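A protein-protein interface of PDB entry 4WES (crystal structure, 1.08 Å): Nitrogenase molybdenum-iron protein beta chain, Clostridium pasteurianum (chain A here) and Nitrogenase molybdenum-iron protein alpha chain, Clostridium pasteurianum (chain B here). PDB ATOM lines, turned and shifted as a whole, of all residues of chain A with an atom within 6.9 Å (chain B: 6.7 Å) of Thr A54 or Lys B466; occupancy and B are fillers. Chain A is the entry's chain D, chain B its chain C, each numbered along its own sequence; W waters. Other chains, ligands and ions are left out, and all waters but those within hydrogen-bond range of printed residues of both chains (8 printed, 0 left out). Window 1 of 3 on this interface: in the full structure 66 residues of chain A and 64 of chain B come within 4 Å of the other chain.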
ATOM      1  N   VAL A  26      -1.808 -15.269 -29.131  1.00  0.00           N
ATOM      2  CA  VAL A  26      -0.850 -14.524 -28.341  1.00  0.00           C
ATOM      3  C   VAL A  26       0.471 -14.352 -29.088  1.00  0.00           C
ATOM      4  O   VAL A  26       1.188 -13.359 -28.882  1.00  0.00           O
ATOM      5  CB  VAL A  26      -0.585 -15.166 -26.956  1.00  0.00           C
ATOM      6  CG1 VAL A  26       0.241 -16.416 -27.019  1.00  0.00           C
ATOM      7  CG2 VAL A  26       0.078 -14.133 -26.034  1.00  0.00           C
ATOM      8  N   MET A  29      -0.136 -11.377 -31.192  1.00  0.00           N
ATOM      9  CA  MET A  29      -0.164 -10.226 -30.306  1.00  0.00           C
ATOM     10  C   MET A  29       1.255  -9.775 -29.943  1.00  0.00           C
ATOM     11  O   MET A  29       1.591  -8.588 -30.027  1.00  0.00           O
ATOM     12  CB  MET A  29      -0.980 -10.559 -29.048  1.00  0.00           C
ATOM     13  CG  MET A  29      -1.156  -9.403 -28.103  1.00  0.00           C
ATOM     14  SD  MET A  29      -2.150  -9.806 -26.659  1.00  0.00           S
ATOM     15  CE  MET A  29      -3.754 -10.011 -27.411  1.00  0.00           C
ATOM     16  N   CYS A  48     -10.533 -14.288 -25.233  1.00  0.00           N
ATOM     17  CA  CYS A  48      -9.243 -14.519 -25.858  1.00  0.00           C
ATOM     18  C   CYS A  48      -8.299 -13.358 -25.554  1.00  0.00           C
ATOM     19  O   CYS A  48      -7.185 -13.548 -25.066  1.00  0.00           O
ATOM     20  CB  CYS A  48      -9.398 -14.690 -27.363  1.00  0.00           C
ATOM     21  SG  CYS A  48     -10.496 -16.039 -27.818  1.00  0.00           S
ATOM     22  N   CYS A  49      -8.732 -12.145 -25.888  1.00  0.00           N
ATOM     23  CA  CYS A  49      -7.867 -10.992 -25.719  1.00  0.00           C
ATOM     24  C   CYS A  49      -7.403 -10.870 -24.278  1.00  0.00           C
ATOM     25  O   CYS A  49      -6.231 -10.596 -23.993  1.00  0.00           O
ATOM     26  CB  CYS A  49      -8.638  -9.737 -26.152  1.00  0.00           C
ATOM     27  SG  CYS A  49      -7.702  -8.204 -26.089  1.00  0.00           S
ATOM     28  N   SER A  50      -8.340 -11.008 -23.336  1.00  0.00           N
ATOM     29  CA  SER A  50      -7.977 -10.891 -21.915  1.00  0.00           C
ATOM     30  C   SER A  50      -6.935 -11.930 -21.515  1.00  0.00           C
ATOM     31  O   SER A  50      -5.941 -11.621 -20.882  1.00  0.00           O
ATOM     32  CB  SER A  50      -9.208 -11.016 -21.027  1.00  0.00           C
ATOM     33  OG  SER A  50      -8.813 -10.805 -19.671  1.00  0.00           O
ATOM     34  N   TYR A  51      -7.175 -13.188 -21.897  1.00  0.00           N
ATOM     35  CA  TYR A  51      -6.225 -14.226 -21.537  1.00  0.00           C
ATOM     36  C   TYR A  51      -4.846 -13.977 -22.140  1.00  0.00           C
ATOM     37  O   TYR A  51      -3.807 -14.275 -21.524  1.00  0.00           O
ATOM     38  CB  TYR A  51      -6.745 -15.586 -21.988  1.00  0.00           C
ATOM     39  CG  TYR A  51      -7.770 -16.285 -21.124  1.00  0.00           C
ATOM     40  CD1 TYR A  51      -7.893 -16.042 -19.753  1.00  0.00           C
ATOM     41  CD2 TYR A  51      -8.593 -17.249 -21.671  1.00  0.00           C
ATOM     42  CE1 TYR A  51      -8.763 -16.797 -18.976  1.00  0.00           C
ATOM     43  CE2 TYR A  51      -9.461 -17.983 -20.908  1.00  0.00           C
ATOM     44  CZ  TYR A  51      -9.572 -17.736 -19.561  1.00  0.00           C
ATOM     45  OH  TYR A  51     -10.442 -18.508 -18.811  1.00  0.00           O
ATOM     46  N   HIS A  52      -4.817 -13.514 -23.395  1.00  0.00           N
ATOM     47  CA  HIS A  52      -3.568 -13.381 -24.132  1.00  0.00           C
ATOM     48  C   HIS A  52      -2.755 -12.186 -23.644  1.00  0.00           C
ATOM     49  O   HIS A  52      -1.544 -12.287 -23.453  1.00  0.00           O
ATOM     50  CB  HIS A  52      -3.844 -13.328 -25.637  1.00  0.00           C
ATOM     51  CG  HIS A  52      -4.599 -14.530 -26.114  1.00  0.00           C
ATOM     52  ND1 HIS A  52      -5.239 -14.585 -27.337  1.00  0.00           N
ATOM     53  CD2 HIS A  52      -4.892 -15.686 -25.464  1.00  0.00           C
ATOM     54  CE1 HIS A  52      -5.880 -15.741 -27.401  1.00  0.00           C
ATOM     55  NE2 HIS A  52      -5.678 -16.438 -26.284  1.00  0.00           N
ATOM     56  N   ARG A  53      -3.441 -11.076 -23.381  1.00  0.00           N
ATOM     57  CA  ARG A  53      -2.779  -9.957 -22.724  1.00  0.00           C
ATOM     58  C   ARG A  53      -2.216 -10.407 -21.379  1.00  0.00           C
ATOM     59  O   ARG A  53      -1.130  -9.996 -20.975  1.00  0.00           O
ATOM     60  CB  ARG A  53      -3.755  -8.820 -22.519  1.00  0.00           C
ATOM     61  CG  ARG A  53      -4.227  -8.131 -23.809  1.00  0.00           C
ATOM     62  CD  ARG A  53      -5.267  -7.066 -23.540  1.00  0.00           C
ATOM     63  NE  ARG A  53      -4.692  -6.011 -22.717  1.00  0.00           N
ATOM     64  CZ  ARG A  53      -5.345  -5.231 -21.868  1.00  0.00           C
ATOM     65  NH1 ARG A  53      -6.649  -5.314 -21.734  1.00  0.00           N
ATOM     66  NH2 ARG A  53      -4.662  -4.388 -21.127  1.00  0.00           N
ATOM     67  N   THR A  54      -3.010 -11.188 -20.651  1.00  0.00           N
ATOM     68  CA  THR A  54      -2.643 -11.589 -19.272  1.00  0.00           C
ATOM     69  C   THR A  54      -1.367 -12.405 -19.242  1.00  0.00           C
ATOM     70  O   THR A  54      -0.505 -12.161 -18.398  1.00  0.00           O
ATOM     71  CB  THR A  54      -3.817 -12.339 -18.629  1.00  0.00           C
ATOM     72  OG1 THR A  54      -4.885 -11.422 -18.400  1.00  0.00           O
ATOM     73  CG2 THR A  54      -3.409 -13.001 -17.328  1.00  0.00           C
ATOM     74  N   VAL A  55      -1.196 -13.371 -20.158  1.00  0.00           N
ATOM     75  CA  VAL A  55      -0.004 -14.192 -20.085  1.00  0.00           C
ATOM     76  C   VAL A  55       1.233 -13.365 -20.372  1.00  0.00           C
ATOM     77  O   VAL A  55       2.287 -13.586 -19.768  1.00  0.00           O
ATOM     78  CB  VAL A  55      -0.101 -15.432 -20.977  1.00  0.00           C
ATOM     79  CG1 VAL A  55      -0.073 -15.104 -22.488  1.00  0.00           C
ATOM     80  CG2 VAL A  55       0.974 -16.446 -20.632  1.00  0.00           C
ATOM     81  N   LEU A  56       1.134 -12.377 -21.267  1.00  0.00           N
ATOM     82  CA  LEU A  56       2.260 -11.498 -21.533  1.00  0.00           C
ATOM     83  C   LEU A  56       2.631 -10.696 -20.304  1.00  0.00           C
ATOM     84  O   LEU A  56       3.831 -10.559 -20.002  1.00  0.00           O
ATOM     85  CB  LEU A  56       1.963 -10.603 -22.747  1.00  0.00           C
ATOM     86  CG  LEU A  56       1.867 -11.341 -24.084  1.00  0.00           C
ATOM     87  CD1 LEU A  56       1.380 -10.413 -25.166  1.00  0.00           C
ATOM     88  CD2 LEU A  56       3.175 -11.961 -24.453  1.00  0.00           C
ATOM     89  N   SER A  57       1.656 -10.164 -19.585  1.00  0.00           N
ATOM     90  CA  SER A  57       1.963  -9.450 -18.357  1.00  0.00           C
ATOM     91  C   SER A  57       2.553 -10.352 -17.277  1.00  0.00           C
ATOM     92  O   SER A  57       3.439  -9.918 -16.529  1.00  0.00           O
ATOM     93  CB  SER A  57       0.764  -8.702 -17.788  1.00  0.00           C
ATOM     94  OG  SER A  57       0.379  -7.620 -18.643  1.00  0.00           O
ATOM     95  N   ARG A  58       2.048 -11.576 -17.157  1.00  0.00           N
ATOM     96  CA  ARG A  58       2.597 -12.510 -16.174  1.00  0.00           C
ATOM     97  C   ARG A  58       4.030 -12.890 -16.455  1.00  0.00           C
ATOM     98  O   ARG A  58       4.812 -13.125 -15.529  1.00  0.00           O
ATOM     99  CB  ARG A  58       1.732 -13.760 -16.083  1.00  0.00           C
ATOM    100  CG  ARG A  58       0.372 -13.525 -15.447  1.00  0.00           C
ATOM    101  CD  ARG A  58      -0.535 -14.747 -15.589  1.00  0.00           C
ATOM    102  NE  ARG A  58      -1.749 -14.563 -14.787  1.00  0.00           N
ATOM    103  CZ  ARG A  58      -2.870 -15.256 -14.947  1.00  0.00           C
ATOM    104  NH1 ARG A  58      -2.958 -16.252 -15.810  1.00  0.00           N
ATOM    105  NH2 ARG A  58      -3.931 -14.930 -14.228  1.00  0.00           N
ATOM    106  N   HIS A  59       4.400 -12.980 -17.746  1.00  0.00           N
ATOM    107  CA  HIS A  59       5.746 -13.347 -18.126  1.00  0.00           C
ATOM    108  C   HIS A  59       6.711 -12.159 -17.955  1.00  0.00           C
ATOM    109  O   HIS A  59       7.777 -12.283 -17.357  1.00  0.00           O
ATOM    110  CB  HIS A  59       5.727 -13.838 -19.576  1.00  0.00           C
ATOM    111  CG  HIS A  59       7.043 -14.161 -20.182  1.00  0.00           C
ATOM    112  ND1 HIS A  59       7.565 -15.427 -20.269  1.00  0.00           N
ATOM    113  CD2 HIS A  59       7.937 -13.345 -20.782  1.00  0.00           C
ATOM    114  CE1 HIS A  59       8.700 -15.373 -20.935  1.00  0.00           C
ATOM    115  NE2 HIS A  59       8.976 -14.118 -21.220  1.00  0.00           N
ATOM    116  N   GLU A  62       5.028  -6.549 -17.157  1.00  0.00           N
ATOM    117  CA  GLU A  62       4.872  -5.290 -17.922  1.00  0.00           C
ATOM    118  C   GLU A  62       3.428  -5.209 -18.372  1.00  0.00           C
ATOM    119  O   GLU A  62       2.756  -6.248 -18.515  1.00  0.00           O
ATOM    120  CB  GLU A  62       5.756  -5.299 -19.183  1.00  0.00           C
ATOM    121  CG  GLU A  62       7.239  -5.153 -18.907  1.00  0.00           C
ATOM    122  CD  GLU A  62       7.574  -3.781 -18.415  1.00  0.00           C
ATOM    123  OE1 GLU A  62       7.683  -3.562 -17.184  1.00  0.00           O
ATOM    124  OE2 GLU A  62       7.765  -2.871 -19.279  1.00  0.00           O
ATOM    125  N   PRO A  63       2.970  -4.004 -18.727  1.00  0.00           N
ATOM    126  CA  PRO A  63       1.718  -3.880 -19.473  1.00  0.00           C
ATOM    127  C   PRO A  63       1.789  -4.615 -20.796  1.00  0.00           C
ATOM    128  O   PRO A  63       2.863  -4.776 -21.375  1.00  0.00           O
ATOM    129  CB  PRO A  63       1.611  -2.381 -19.721  1.00  0.00           C
ATOM    130  CG  PRO A  63       2.474  -1.761 -18.666  1.00  0.00           C
ATOM    131  CD  PRO A  63       3.631  -2.699 -18.563  1.00  0.00           C
ATOM    132  N   ALA A  64       0.621  -5.005 -21.311  1.00  0.00           N
ATOM    133  CA  ALA A  64       0.526  -5.604 -22.636  1.00  0.00           C
ATOM    134  C   ALA A  64      -0.854  -5.238 -23.170  1.00  0.00           C
ATOM    135  O   ALA A  64      -1.841  -5.862 -22.805  1.00  0.00           O
ATOM    136  CB  ALA A  64       0.753  -7.110 -22.609  1.00  0.00           C
ATOM    137  N   MET A  65      -0.889  -4.210 -24.000  1.00  0.00           N
ATOM    138  CA  MET A  65      -2.130  -3.622 -24.516  1.00  0.00           C
ATOM    139  C   MET A  65      -2.637  -4.341 -25.744  1.00  0.00           C
ATOM    140  O   MET A  65      -1.876  -4.677 -26.635  1.00  0.00           O
ATOM    141  CB  MET A  65      -1.889  -2.179 -24.902  1.00  0.00           C
ATOM    142  CG  MET A  65      -1.860  -1.273 -23.707  1.00  0.00           C
ATOM    143  SD  MET A  65      -3.518  -1.101 -23.044  1.00  0.00           S
ATOM    144  CE  MET A  65      -3.204  -0.835 -21.317  1.00  0.00           C
ATOM    145  N   MET A 414       6.660 -17.205 -15.606  1.00  0.00           N
ATOM    146  CA  MET A 414       5.734 -16.309 -14.916  1.00  0.00           C
ATOM    147  C   MET A 414       6.000 -16.182 -13.422  1.00  0.00           C
ATOM    148  O   MET A 414       5.226 -15.571 -12.705  1.00  0.00           O
ATOM    149  CB  MET A 414       4.290 -16.776 -15.125  1.00  0.00           C
ATOM    150  CG  MET A 414       3.891 -16.823 -16.580  1.00  0.00           C
ATOM    151  SD  MET A 414       2.198 -17.336 -16.870  1.00  0.00           S
ATOM    152  CE  MET A 414       2.232 -19.056 -16.431  1.00  0.00           C
ATOM    153  N   THR B  49     -11.357  -3.245 -22.670  1.00  0.00           N
ATOM    154  CA  THR B  49     -12.077  -3.760 -21.523  1.00  0.00           C
ATOM    155  C   THR B  49     -11.161  -4.663 -20.718  1.00  0.00           C
ATOM    156  O   THR B  49     -10.168  -5.177 -21.233  1.00  0.00           O
ATOM    157  CB  THR B  49     -13.320  -4.563 -21.976  1.00  0.00           C
ATOM    158  OG1 THR B  49     -14.081  -4.990 -20.849  1.00  0.00           O
ATOM    159  CG2 THR B  49     -12.965  -5.743 -22.811  1.00  0.00           C
ATOM    160  N   ALA B  50     -11.519  -4.919 -19.454  1.00  0.00           N
ATOM    161  CA  ALA B  50     -10.866  -5.958 -18.674  1.00  0.00           C
ATOM    162  C   ALA B  50     -11.629  -7.282 -18.714  1.00  0.00           C
ATOM    163  O   ALA B  50     -11.128  -8.288 -18.218  1.00  0.00           O
ATOM    164  CB  ALA B  50     -10.726  -5.508 -17.237  1.00  0.00           C
ATOM    165  N   ARG B  51     -12.839  -7.280 -19.282  1.00  0.00           N
ATOM    166  CA  ARG B  51     -13.724  -8.448 -19.261  1.00  0.00           C
ATOM    167  C   ARG B  51     -13.178  -9.682 -19.938  1.00  0.00           C
ATOM    168  O   ARG B  51     -12.419  -9.617 -20.907  1.00  0.00           O
ATOM    169  CB  ARG B  51     -15.049  -8.081 -19.954  1.00  0.00           C
ATOM    170  CG  ARG B  51     -15.965  -7.231 -19.140  1.00  0.00           C
ATOM    171  CD  ARG B  51     -17.135  -6.782 -19.977  1.00  0.00           C
ATOM    172  NE  ARG B  51     -18.209  -6.284 -19.154  1.00  0.00           N
ATOM    173  CZ  ARG B  51     -19.422  -5.966 -19.591  1.00  0.00           C
ATOM    174  NH1 ARG B  51     -19.697  -6.051 -20.871  1.00  0.00           N
ATOM    175  NH2 ARG B  51     -20.355  -5.589 -18.733  1.00  0.00           N
ATOM    176  N   GLY B  52     -13.655 -10.827 -19.422  1.00  0.00           N
ATOM    177  CA  GLY B  52     -13.478 -12.121 -20.069  1.00  0.00           C
ATOM    178  C   GLY B  52     -14.770 -12.653 -20.626  1.00  0.00           C
ATOM    179  O   GLY B  52     -15.690 -11.905 -20.923  1.00  0.00           O
ATOM    180  N   TYR B  82      -5.077 -21.381 -20.664  1.00  0.00           N
ATOM    181  CA  TYR B  82      -5.271 -20.162 -19.879  1.00  0.00           C
ATOM    182  C   TYR B  82      -6.055 -20.355 -18.594  1.00  0.00           C
ATOM    183  O   TYR B  82      -6.230 -19.407 -17.825  1.00  0.00           O
ATOM    184  CB  TYR B  82      -5.830 -19.055 -20.790  1.00  0.00           C
ATOM    185  CG  TYR B  82      -4.857 -18.684 -21.862  1.00  0.00           C
ATOM    186  CD1 TYR B  82      -3.623 -18.139 -21.545  1.00  0.00           C
ATOM    187  CD2 TYR B  82      -5.126 -18.900 -23.201  1.00  0.00           C
ATOM    188  CE1 TYR B  82      -2.691 -17.812 -22.500  1.00  0.00           C
ATOM    189  CE2 TYR B  82      -4.161 -18.583 -24.183  1.00  0.00           C
ATOM    190  CZ  TYR B  82      -2.954 -18.043 -23.833  1.00  0.00           C
ATOM    191  OH  TYR B  82      -1.992 -17.701 -24.761  1.00  0.00           O
ATOM    192  N   GLU B 368     -16.322  -5.132 -13.451  1.00  0.00           N
ATOM    193  CA  GLU B 368     -16.298  -5.552 -14.841  1.00  0.00           C
ATOM    194  C   GLU B 368     -17.676  -5.953 -15.332  1.00  0.00           C
ATOM    195  O   GLU B 368     -18.050  -5.608 -16.449  1.00  0.00           O
ATOM    196  CB  GLU B 368     -15.376  -6.765 -15.018  1.00  0.00           C
ATOM    197  CG  GLU B 368     -13.882  -6.549 -14.813  1.00  0.00           C
ATOM    198  CD  GLU B 368     -13.039  -7.765 -15.073  1.00  0.00           C
ATOM    199  OE1 GLU B 368     -11.836  -7.759 -14.628  1.00  0.00           O
ATOM    200  OE2 GLU B 368     -13.490  -8.704 -15.760  1.00  0.00           O
ATOM    201  N   MET B 449      -9.823   4.773 -16.813  1.00  0.00           N
ATOM    202  CA  MET B 449      -8.872   4.640 -15.715  1.00  0.00           C
ATOM    203  C   MET B 449      -7.819   5.738 -15.751  1.00  0.00           C
ATOM    204  O   MET B 449      -7.471   6.299 -14.710  1.00  0.00           O
ATOM    205  CB  MET B 449      -8.207   3.270 -15.760  1.00  0.00           C
ATOM    206  CG  MET B 449      -7.431   2.973 -14.493  1.00  0.00           C
ATOM    207  SD  MET B 449      -6.527   1.412 -14.546  1.00  0.00           S
ATOM    208  CE  MET B 449      -5.235   1.862 -15.694  1.00  0.00           C
ATOM    209  N   ALA B 463      -6.843  -3.517  -8.578  1.00  0.00           N
ATOM    210  CA  ALA B 463      -7.455  -4.012  -9.809  1.00  0.00           C
ATOM    211  C   ALA B 463      -6.942  -5.430 -10.064  1.00  0.00           C
ATOM    212  O   ALA B 463      -6.883  -6.258  -9.129  1.00  0.00           O
ATOM    213  CB  ALA B 463      -7.190  -3.039 -10.962  1.00  0.00           C
ATOM    214  N   GLY B 464      -6.592  -5.743 -11.307  1.00  0.00           N
ATOM    215  CA  GLY B 464      -6.100  -7.037 -11.692  1.00  0.00           C
ATOM    216  C   GLY B 464      -4.779  -6.953 -12.417  1.00  0.00           C
ATOM    217  O   GLY B 464      -4.095  -5.922 -12.397  1.00  0.00           O
ATOM    218  N   ILE B 465      -4.409  -8.047 -13.077  1.00  0.00           N
ATOM    219  CA  ILE B 465      -3.089  -8.163 -13.673  1.00  0.00           C
ATOM    220  C   ILE B 465      -2.915  -7.301 -14.919  1.00  0.00           C
ATOM    221  O   ILE B 465      -1.809  -6.868 -15.217  1.00  0.00           O
ATOM    222  CB  ILE B 465      -2.809  -9.662 -13.996  1.00  0.00           C
ATOM    223  CG1 ILE B 465      -1.368  -9.920 -14.378  1.00  0.00           C
ATOM    224  CG2 ILE B 465      -3.736 -10.205 -15.080  1.00  0.00           C
ATOM    225  CD1 ILE B 465      -0.345  -9.520 -13.352  1.00  0.00           C
ATOM    226  N   LYS B 466      -3.995  -7.054 -15.651  1.00  0.00           N
ATOM    227  CA  LYS B 466      -3.883  -6.265 -16.880  1.00  0.00           C
ATOM    228  C   LYS B 466      -3.699  -4.790 -16.550  1.00  0.00           C
ATOM    229  O   LYS B 466      -3.024  -4.045 -17.288  1.00  0.00           O
ATOM    230  CB  LYS B 466      -5.074  -6.498 -17.808  1.00  0.00           C
ATOM    231  CG  LYS B 466      -5.259  -7.946 -18.213  1.00  0.00           C
ATOM    232  CD  LYS B 466      -6.271  -8.167 -19.331  1.00  0.00           C
ATOM    233  CE  LYS B 466      -7.694  -7.747 -19.002  1.00  0.00           C
ATOM    234  NZ  LYS B 466      -8.251  -8.414 -17.783  1.00  0.00           N
ATOM    235  N   GLU B 467      -4.307  -4.318 -15.449  1.00  0.00           N
ATOM    236  CA  GLU B 467      -4.188  -2.915 -15.058  1.00  0.00           C
ATOM    237  C   GLU B 467      -2.945  -2.661 -14.189  1.00  0.00           C
ATOM    238  O   GLU B 467      -2.417  -1.546 -14.185  1.00  0.00           O
ATOM    239  CB  GLU B 467      -5.398  -2.479 -14.252  1.00  0.00           C
ATOM    240  CG  GLU B 467      -6.745  -2.687 -14.929  1.00  0.00           C
ATOM    241  CD  GLU B 467      -7.456  -3.997 -14.618  1.00  0.00           C
ATOM    242  OE1 GLU B 467      -8.705  -4.028 -14.779  1.00  0.00           O
ATOM    243  OE2 GLU B 467      -6.775  -4.969 -14.172  1.00  0.00           O
ATOM    244  N   LYS B 468      -2.485  -3.669 -13.449  1.00  0.00           N
ATOM    245  CA  LYS B 468      -1.487  -3.448 -12.396  1.00  0.00           C
ATOM    246  C   LYS B 468      -0.293  -2.640 -12.890  1.00  0.00           C
ATOM    247  O   LYS B 468       0.084  -1.615 -12.281  1.00  0.00           O
ATOM    248  CB  LYS B 468      -0.973  -4.763 -11.810  1.00  0.00           C
ATOM    249  CG  LYS B 468       0.043  -4.555 -10.688  1.00  0.00           C
ATOM    250  CD  LYS B 468       0.715  -5.828 -10.256  1.00  0.00           C
ATOM    251  CE  LYS B 468       1.749  -5.646  -9.179  1.00  0.00           C
ATOM    252  NZ  LYS B 468       1.154  -5.484  -7.818  1.00  0.00           N
ATOM    253  N   PHE B 469       0.369  -3.100 -13.939  1.00  0.00           N
ATOM    254  CA  PHE B 469       1.612  -2.468 -14.352  1.00  0.00           C
ATOM    255  C   PHE B 469       1.368  -1.160 -15.084  1.00  0.00           C
ATOM    256  O   PHE B 469       2.222  -0.277 -15.077  1.00  0.00           O
ATOM    257  CB  PHE B 469       2.469  -3.442 -15.158  1.00  0.00           C
ATOM    258  CG  PHE B 469       2.822  -4.687 -14.375  1.00  0.00           C
ATOM    259  CD1 PHE B 469       3.593  -4.596 -13.241  1.00  0.00           C
ATOM    260  CD2 PHE B 469       2.352  -5.915 -14.763  1.00  0.00           C
ATOM    261  CE1 PHE B 469       3.909  -5.725 -12.498  1.00  0.00           C
ATOM    262  CE2 PHE B 469       2.628  -7.059 -14.016  1.00  0.00           C
ATOM    263  CZ  PHE B 469       3.408  -6.947 -12.884  1.00  0.00           C
ATOM    264  N   VAL B 470       0.188  -0.995 -15.683  1.00  0.00           N
ATOM    265  CA  VAL B 470      -0.170   0.281 -16.295  1.00  0.00           C
ATOM    266  C   VAL B 470      -0.168   1.360 -15.199  1.00  0.00           C
ATOM    267  O   VAL B 470       0.396   2.448 -15.366  1.00  0.00           O
ATOM    268  CB  VAL B 470      -1.567   0.203 -16.968  1.00  0.00           C
ATOM    269  CG1 VAL B 470      -2.028   1.584 -17.402  1.00  0.00           C
ATOM    270  CG2 VAL B 470      -1.543  -0.760 -18.145  1.00  0.00           C
ATOM    271  N   ILE B 471      -0.826   1.048 -14.091  1.00  0.00           N
ATOM    272  CA  ILE B 471      -0.925   1.949 -12.958  1.00  0.00           C
ATOM    273  C   ILE B 471       0.440   2.194 -12.352  1.00  0.00           C
ATOM    274  O   ILE B 471       0.833   3.358 -12.096  1.00  0.00           O
ATOM    275  CB  ILE B 471      -1.897   1.374 -11.897  1.00  0.00           C
ATOM    276  CG1 ILE B 471      -3.319   1.247 -12.464  1.00  0.00           C
ATOM    277  CG2 ILE B 471      -1.861   2.215 -10.632  1.00  0.00           C
ATOM    278  CD1 ILE B 471      -4.177   0.237 -11.720  1.00  0.00           C
ATOM    279  N   GLN B 480      -3.300  -6.272  -6.572  1.00  0.00           N
ATOM    280  CA  GLN B 480      -4.288  -7.087  -7.244  1.00  0.00           C
ATOM    281  C   GLN B 480      -5.307  -7.664  -6.278  1.00  0.00           C
ATOM    282  O   GLN B 480      -4.926  -8.368  -5.324  1.00  0.00           O
ATOM    283  CB  GLN B 480      -3.562  -8.255  -7.924  1.00  0.00           C
ATOM    284  CG  GLN B 480      -2.591  -7.853  -9.009  1.00  0.00           C
ATOM    285  CD  GLN B 480      -1.984  -9.062  -9.703  1.00  0.00           C
ATOM    286  OE1 GLN B 480      -2.679  -9.783 -10.423  1.00  0.00           O
ATOM    287  NE2 GLN B 480      -0.730  -9.348  -9.440  1.00  0.00           N
ATOM    288  N   HIS B 482      -7.733  -9.747  -7.407  1.00  0.00           N
ATOM    289  CA  HIS B 482      -8.101 -11.102  -7.857  1.00  0.00           C
ATOM    290  C   HIS B 482      -7.084 -12.104  -7.312  1.00  0.00           C
ATOM    291  O   HIS B 482      -7.418 -12.986  -6.514  1.00  0.00           O
ATOM    292  CB  HIS B 482      -8.183 -11.251  -9.394  1.00  0.00           C
ATOM    293  CG  HIS B 482      -9.005 -10.243 -10.133  1.00  0.00           C
ATOM    294  ND1 HIS B 482     -10.131 -10.574 -10.851  1.00  0.00           N
ATOM    295  CD2 HIS B 482      -8.740  -8.954 -10.442  1.00  0.00           C
ATOM    296  CE1 HIS B 482     -10.544  -9.538 -11.543  1.00  0.00           C
ATOM    297  NE2 HIS B 482      -9.703  -8.540 -11.314  1.00  0.00           N
HETATM  298  O   HOH W   1      -7.522  -4.236 -19.206  1.00  0.00           O
HETATM  299  O   HOH W   2      -5.129  -2.767 -18.811  1.00  0.00           O
HETATM  300  O   HOH W   3      -8.942  -7.044 -22.831  1.00  0.00           O
HETATM  301  O   HOH W   4      -1.947  -4.706 -19.881  1.00  0.00           O
HETATM  302  O   HOH W   5      -7.177 -10.922 -16.998  1.00  0.00           O
HETATM  303  O   HOH W   6      -2.719 -17.594 -27.412  1.00  0.00           O
HETATM  304  O   HOH W   7     -10.672 -11.018 -17.661  1.00  0.00           O
HETATM  305  O   HOH W   8      -5.208 -16.835 -17.533  1.00  0.00           O
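The side-chain hydroxyl (OG) of Ser A50 is in hydrogen-bond range of the side-chain amino group (NZ) of Lys B466, 3.1 Å away.
The side-chain hydroxyl of Thr B49 lies within hydrogen-bond range of the backbone NH of Arg B51 (3.0 Å).
The backbone NH of Arg A53 is in hydrogen-bond range of the side-chain sulfur of Met A29 (3.7 Å).
The side-chain hydroxyl of Ser A57 sits at hydrogen-bond distance from the backbone carbonyl oxygen of Glu A62, 2.7 Å away.
The backbone carbonyl oxygen (O) of Ala B50 lies within hydrogen-bond range of the side-chain amino group (NZ) of Lys B466, 2.9 Å away.
The backbone carbonyl oxygen of Cys A48 lies close to a ring nitrogen (ND1) of His A52 (3.2 Å).
NE of Arg A53 lies within hydrogen-bond range of O of Ala A64 (2.9 Å).
Tyr B82 touches Val A26.
Ser A50 touches Ala B50 (OG to O, 3.7 Å).
Ser A50 touches Arg B51 (CB to O, 3.5 Å).
His A52 touches Tyr B82 (CD2 to CE2, 3.3 Å).
Thr A54 touches Ile B465 (CG2 to CG2, 3.6 Å).
OG1 of Thr A54 touches CG of Lys B466 (3.5 Å).
CE1 of Tyr B82 touches CG1 of Val A55, 3.8 Å away.
Ser A57 touches Phe B469 (O to CE2, 3.9 Å).
N of Glu A62 touches CD2 of Phe B469, 3.6 Å away.
Met A65 touches Val B470.
Of the printed residues of chain B, Val A26 touches Tyr B82.
Of the printed residues of chain B, Ser A50 touches Ala B50, Arg B51 and Lys B466.
Of chain B, only Ile B465 and Lys B466 come within 4 Å of Thr A54.
Printed residues of chain B within 4 Å of Ser A57: Phe B469.
Of the printed residues of chain B, Met A65 touches Val B470 (3.6 Å).
Met B449 touches none of the printed residues of chain A.
Of the printed residues of chain A, Ile B465 touches Thr A54.
Of the printed residues of chain A, Lys B466 touches Ser A50, Arg A53 and Thr A54.
The nearest residue of chain B that does not touch Thr A54 is Tyr B82 (6.5 Å).
The nearest printed residue of chain A that does not touch Lys B466 is Ser A57 (4.8 Å).
The nearest printed residue of chain B that does not touch Val A55 is Ile B465 (6.5 Å).
Along chain B the printed residues that touch a printed residue of chain A span positions 49 to 470.
Hydrophobic or aromatic side chains of chain A that line the printed part of chain B: Val A26, Tyr A51, His A52, Val A55, Pro A63 and Met A65.
Water W5 lies within hydrogen-bond range of OG1 of Thr A54 (2.7 Å), NZ of Lys B466 (2.8 Å) and OG of Ser A50 (3.1 Å).
Water W3 lies within hydrogen-bond range of the backbone carbonyl oxygen of Thr B49, the guanidinium group of Arg A53 and the side-chain sulfur of Cys A49.
Water W7 lies within hydrogen-bond range of the side-chain hydroxyl of Ser A50 (2.7 Å), the backbone carbonyl oxygen of Ala B50 (2.8 Å) and the backbone NH of Gly B52 (3.5 Å).
Water W6 lies within hydrogen-bond range of OH of Tyr B82 (2.8 Å), N of Val A26 (3.0 Å) and NE2 of His A52 (3.4 Å).
Water W2 lies within hydrogen-bond range of the guanidinium group (NH2) of Arg A53 (2.9 Å) and the backbone carbonyl oxygen (O) of Lys B466 (2.9 Å).
Water W4 lies within hydrogen-bond range of the backbone carbonyl oxygen of Lys B466 (2.9 Å), the backbone NH of Ala A64 (3.0 Å) and the guanidinium group of Arg A53 (3.0 Å).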
